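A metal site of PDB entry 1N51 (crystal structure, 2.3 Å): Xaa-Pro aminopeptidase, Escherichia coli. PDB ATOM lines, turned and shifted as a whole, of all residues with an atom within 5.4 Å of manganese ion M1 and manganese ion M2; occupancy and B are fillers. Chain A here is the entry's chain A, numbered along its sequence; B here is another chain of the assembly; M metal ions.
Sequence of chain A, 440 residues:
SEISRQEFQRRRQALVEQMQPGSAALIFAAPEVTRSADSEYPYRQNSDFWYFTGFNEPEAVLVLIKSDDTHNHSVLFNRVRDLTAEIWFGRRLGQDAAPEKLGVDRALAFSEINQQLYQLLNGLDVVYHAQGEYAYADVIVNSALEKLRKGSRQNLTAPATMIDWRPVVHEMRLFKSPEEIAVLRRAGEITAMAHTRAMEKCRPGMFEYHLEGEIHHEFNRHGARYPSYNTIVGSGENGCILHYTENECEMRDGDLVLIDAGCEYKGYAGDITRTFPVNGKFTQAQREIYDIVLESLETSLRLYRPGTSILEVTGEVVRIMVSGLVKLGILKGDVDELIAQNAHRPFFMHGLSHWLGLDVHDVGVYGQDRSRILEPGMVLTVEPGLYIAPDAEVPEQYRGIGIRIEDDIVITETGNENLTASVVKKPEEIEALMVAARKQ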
ATOM      1  N   TYR A 229      12.767   3.411   8.421  1.00  0.00           N
ATOM      2  CA  TYR A 229      12.033   2.146   8.587  1.00  0.00           C
ATOM      3  C   TYR A 229      11.317   1.855   7.274  1.00  0.00           C
ATOM      4  O   TYR A 229      11.149   2.753   6.451  1.00  0.00           O
ATOM      5  CB  TYR A 229      11.019   2.214   9.734  1.00  0.00           C
ATOM      6  CG  TYR A 229      10.039   3.358   9.641  1.00  0.00           C
ATOM      7  CD1 TYR A 229      10.367   4.611  10.162  1.00  0.00           C
ATOM      8  CD2 TYR A 229       8.805   3.218   8.992  1.00  0.00           C
ATOM      9  CE1 TYR A 229       9.491   5.698  10.044  1.00  0.00           C
ATOM     10  CE2 TYR A 229       7.930   4.285   8.864  1.00  0.00           C
ATOM     11  CZ  TYR A 229       8.275   5.530   9.400  1.00  0.00           C
ATOM     12  OH  TYR A 229       7.423   6.611   9.285  1.00  0.00           O
ATOM     13  N   ASP A 260       2.747   5.605   6.247  1.00  0.00           N
ATOM     14  CA  ASP A 260       3.610   5.790   7.394  1.00  0.00           C
ATOM     15  C   ASP A 260       5.014   5.679   6.804  1.00  0.00           C
ATOM     16  O   ASP A 260       5.439   4.600   6.383  1.00  0.00           O
ATOM     17  CB  ASP A 260       3.376   4.701   8.435  1.00  0.00           C
ATOM     18  CG  ASP A 260       3.942   5.067   9.809  1.00  0.00           C
ATOM     19  OD1 ASP A 260       4.817   5.956   9.901  1.00  0.00           O
ATOM     20  OD2 ASP A 260       3.527   4.437  10.805  1.00  0.00           O
ATOM     21  N   ASP A 271       9.338  10.395  11.369  1.00  0.00           N
ATOM     22  CA  ASP A 271       8.310   9.361  11.468  1.00  0.00           C
ATOM     23  C   ASP A 271       6.940   9.990  11.369  1.00  0.00           C
ATOM     24  O   ASP A 271       6.376  10.438  12.362  1.00  0.00           O
ATOM     25  CB  ASP A 271       8.440   8.610  12.801  1.00  0.00           C
ATOM     26  CG  ASP A 271       7.425   7.483  12.935  1.00  0.00           C
ATOM     27  OD1 ASP A 271       6.664   7.240  11.964  1.00  0.00           O
ATOM     28  OD2 ASP A 271       7.381   6.833  14.001  1.00  0.00           O
ATOM     29  N   ILE A 272       6.398  10.035  10.157  1.00  0.00           N
ATOM     30  CA  ILE A 272       5.094  10.628   9.932  1.00  0.00           C
ATOM     31  C   ILE A 272       4.086   9.650   9.312  1.00  0.00           C
ATOM     32  O   ILE A 272       4.433   8.788   8.502  1.00  0.00           O
ATOM     33  CB  ILE A 272       5.204  11.847   8.977  1.00  0.00           C
ATOM     34  CG1 ILE A 272       5.967  12.982   9.659  1.00  0.00           C
ATOM     35  CG2 ILE A 272       3.804  12.306   8.547  1.00  0.00           C
ATOM     36  CD1 ILE A 272       6.246  14.162   8.733  1.00  0.00           C
ATOM     37  N   THR A 273       2.834   9.801   9.728  1.00  0.00           N
ATOM     38  CA  THR A 273       1.747   9.014   9.181  1.00  0.00           C
ATOM     39  C   THR A 273       0.660   9.990   8.781  1.00  0.00           C
ATOM     40  O   THR A 273       0.288  10.880   9.568  1.00  0.00           O
ATOM     41  CB  THR A 273       1.133   8.002  10.167  1.00  0.00           C
ATOM     42  OG1 THR A 273       2.120   7.080  10.632  1.00  0.00           O
ATOM     43  CG2 THR A 273       0.025   7.218   9.448  1.00  0.00           C
ATOM     44  N   HIS A 354       5.997   6.913  21.160  1.00  0.00           N
ATOM     45  CA  HIS A 354       7.236   6.189  21.414  1.00  0.00           C
ATOM     46  C   HIS A 354       8.380   7.183  21.245  1.00  0.00           C
ATOM     47  O   HIS A 354       8.252   8.173  20.517  1.00  0.00           O
ATOM     48  CB  HIS A 354       7.402   4.995  20.453  1.00  0.00           C
ATOM     49  CG  HIS A 354       7.471   5.359  19.002  1.00  0.00           C
ATOM     50  ND1 HIS A 354       8.541   5.979  18.405  1.00  0.00           N
ATOM     51  CD2 HIS A 354       6.565   5.149  18.005  1.00  0.00           C
ATOM     52  CE1 HIS A 354       8.267   6.131  17.100  1.00  0.00           C
ATOM     53  NE2 HIS A 354       7.078   5.647  16.805  1.00  0.00           N
ATOM     54  N   VAL A 360      13.947   4.782  15.091  1.00  0.00           N
ATOM     55  CA  VAL A 360      12.569   5.240  15.042  1.00  0.00           C
ATOM     56  C   VAL A 360      11.855   4.914  16.354  1.00  0.00           C
ATOM     57  O   VAL A 360      11.143   5.744  16.902  1.00  0.00           O
ATOM     58  CB  VAL A 360      11.834   4.680  13.801  1.00  0.00           C
ATOM     59  CG1 VAL A 360      11.808   3.161  13.827  1.00  0.00           C
ATOM     60  CG2 VAL A 360      10.436   5.270  13.721  1.00  0.00           C
ATOM     61  N   HIS A 361      12.035   3.690  16.859  1.00  0.00           N
ATOM     62  CA  HIS A 361      11.466   3.335  18.165  1.00  0.00           C
ATOM     63  C   HIS A 361      12.679   3.487  19.062  1.00  0.00           C
ATOM     64  O   HIS A 361      13.364   2.514  19.381  1.00  0.00           O
ATOM     65  CB  HIS A 361      11.019   1.868  18.191  1.00  0.00           C
ATOM     66  CG  HIS A 361       9.769   1.605  17.397  1.00  0.00           C
ATOM     67  ND1 HIS A 361       9.350   0.333  17.083  1.00  0.00           N
ATOM     68  CD2 HIS A 361       8.849   2.445  16.876  1.00  0.00           C
ATOM     69  CE1 HIS A 361       8.223   0.405  16.396  1.00  0.00           C
ATOM     70  NE2 HIS A 361       7.901   1.674  16.264  1.00  0.00           N
ATOM     71  N   THR A 381       6.737  10.559  19.383  1.00  0.00           N
ATOM     72  CA  THR A 381       5.717  10.627  18.347  1.00  0.00           C
ATOM     73  C   THR A 381       4.351  10.718  19.008  1.00  0.00           C
ATOM     74  O   THR A 381       4.190  10.423  20.185  1.00  0.00           O
ATOM     75  CB  THR A 381       5.721   9.349  17.456  1.00  0.00           C
ATOM     76  OG1 THR A 381       5.369   8.207  18.249  1.00  0.00           O
ATOM     77  CG2 THR A 381       7.104   9.141  16.859  1.00  0.00           C
ATOM     78  N   GLU A 383       0.758   9.410  17.746  1.00  0.00           N
ATOM     79  CA  GLU A 383       0.105   8.709  16.653  1.00  0.00           C
ATOM     80  C   GLU A 383      -1.176   7.932  16.936  1.00  0.00           C
ATOM     81  O   GLU A 383      -1.187   6.703  16.860  1.00  0.00           O
ATOM     82  CB  GLU A 383       1.115   7.781  15.986  1.00  0.00           C
ATOM     83  CG  GLU A 383       1.805   6.826  16.955  1.00  0.00           C
ATOM     84  CD  GLU A 383       2.904   6.020  16.285  1.00  0.00           C
ATOM     85  OE1 GLU A 383       2.593   5.353  15.282  1.00  0.00           O
ATOM     86  OE2 GLU A 383       4.066   6.050  16.753  1.00  0.00           O
ATOM     87  N   ARG A 404      -4.558   6.569  10.667  1.00  0.00           N
ATOM     88  CA  ARG A 404      -3.570   6.940  11.675  1.00  0.00           C
ATOM     89  C   ARG A 404      -2.991   8.270  11.235  1.00  0.00           C
ATOM     90  O   ARG A 404      -2.755   8.501  10.042  1.00  0.00           O
ATOM     91  CB  ARG A 404      -2.454   5.894  11.800  1.00  0.00           C
ATOM     92  CG  ARG A 404      -1.315   6.345  12.730  1.00  0.00           C
ATOM     93  CD  ARG A 404      -0.382   5.206  13.195  1.00  0.00           C
ATOM     94  NE  ARG A 404       0.480   4.685  12.136  1.00  0.00           N
ATOM     95  CZ  ARG A 404       0.277   3.532  11.505  1.00  0.00           C
ATOM     96  NH1 ARG A 404      -0.757   2.763  11.824  1.00  0.00           N
ATOM     97  NH2 ARG A 404       1.124   3.130  10.560  1.00  0.00           N
ATOM     98  N   GLU A 406       0.131  10.754  12.472  1.00  0.00           N
ATOM     99  CA  GLU A 406       1.264  10.837  13.372  1.00  0.00           C
ATOM    100  C   GLU A 406       2.230  11.994  13.139  1.00  0.00           C
ATOM    101  O   GLU A 406       2.658  12.229  12.011  1.00  0.00           O
ATOM    102  CB  GLU A 406       2.016   9.505  13.312  1.00  0.00           C
ATOM    103  CG  GLU A 406       3.478   9.541  13.747  1.00  0.00           C
ATOM    104  CD  GLU A 406       4.152   8.184  13.659  1.00  0.00           C
ATOM    105  OE1 GLU A 406       3.938   7.489  12.635  1.00  0.00           O
ATOM    106  OE2 GLU A 406       4.894   7.809  14.597  1.00  0.00           O
ATOM    107  CB  01B B   1       6.352   3.011  12.788  1.00  0.00           C
ATOM    108  CA  01B B   1       5.015   3.474  13.388  1.00  0.00           C
ATOM    109  N   01B B   1       6.745   3.897  11.648  1.00  0.00           N
ATOM    110  O2  01B B   1       5.042   4.892  13.663  1.00  0.00           O
ATOM    111  C   01B B   1       4.714   2.716  14.680  1.00  0.00           C
ATOM    112  C6  01B B   1       6.229   1.551  12.311  1.00  0.00           C
ATOM    113  C7  01B B   1       7.550   0.819  12.201  1.00  0.00           C
ATOM    114  C8  01B B   1       7.795  -0.049  11.130  1.00  0.00           C
ATOM    115  C9  01B B   1       8.971  -0.796  11.067  1.00  0.00           C
ATOM    116  C10 01B B   1       9.929  -0.690  12.076  1.00  0.00           C
ATOM    117  C11 01B B   1       9.704   0.174  13.141  1.00  0.00           C
ATOM    118  C12 01B B   1       8.515   0.919  13.197  1.00  0.00           C
ATOM    119  O   01B B   1       5.555   2.624  15.574  1.00  0.00           O
ATOM    120  N   PRO B   2       3.493   2.164  14.782  1.00  0.00           N
ATOM    121  CA  PRO B   2       3.031   1.414  15.948  1.00  0.00           C
ATOM    122  C   PRO B   2       4.096   0.561  16.611  1.00  0.00           C
ATOM    123  O   PRO B   2       4.556  -0.436  16.055  1.00  0.00           O
ATOM    124  CB  PRO B   2       1.880   0.605  15.379  1.00  0.00           C
ATOM    125  CG  PRO B   2       1.256   1.592  14.442  1.00  0.00           C
ATOM    126  CD  PRO B   2       2.465   2.141  13.714  1.00  0.00           C
HETATM  127 MN    MN M   1       5.838   6.202  15.244  1.00  0.00          MN
HETATM  128 MN    MN M   2       5.130   5.842  12.046  1.00  0.00          MN
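Thr 381 touches manganese ion M1 (CG2 to MN, 3.6 Å). Of the 14 residues printed, 6 come within 4 Å of manganese ion M1. The nearest printed residue that does not touch manganese ion M1 is Pro 2 of chain B (4.7 Å).
N of Glu 406 sits at hydrogen-bond distance from O of Thr 273, at 2.9 Å. The backbone carbonyl oxygen (O) of Val 360 lies close to a ring nitrogen (ND1) of His 354 (3.0 Å). OG1 of Thr 273 sits close to OD2 of Asp 260. OD1 of Asp 260 lies close to OH of Tyr 229 (2.8 Å). The guanidinium group of Arg 404 sits close to the side-chain carboxylate of Asp 260 (2.7 Å). The side-chain carboxylate (OE2) of Glu 383 sits close to the side-chain hydroxyl (OG1) of Thr 381, at 2.9 Å. OE1 of Glu 383 is in salt-bridge range of NE of Arg 404 (3.8 Å). OG1 of Thr 273 is in hydrogen-bond range of NE of Arg 404 (3.3 Å).
Manganese ion M2 is bound by O2 of 01B 1 of chain B (1.9 Å). OD1 of Asp 271 binds manganese ion M2 (2.1 Å). Manganese ion M2 is bound by OE1 of Glu 406, 2.1 Å away. Manganese ion M2 is bound by OD1 of Asp 260. Manganese ion M2 is bound by OD2 of Asp 260 (2.5 Å). N of 01B 1 of chain B is bound to manganese ion M2 (2.6 Å). Manganese ion M2 has six donor atoms within binding distance.
Manganese ion M1 is bound by OE2 of Glu 406, NE2 of His 354, OD2 of Asp 271, O2 of 01B 1 of chain B and OE2 of Glu 383.
OH of Tyr 229 touches manganese ion M2, at 3.7 Å. Thr 273 touches manganese ion M2 (OG1 to MN, 3.5 Å). Six residues have an atom within 4 Å of manganese ion M2: Tyr 229, Asp 260, Asp 271, Thr 273, Glu 406 and 01B 1 of chain B.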
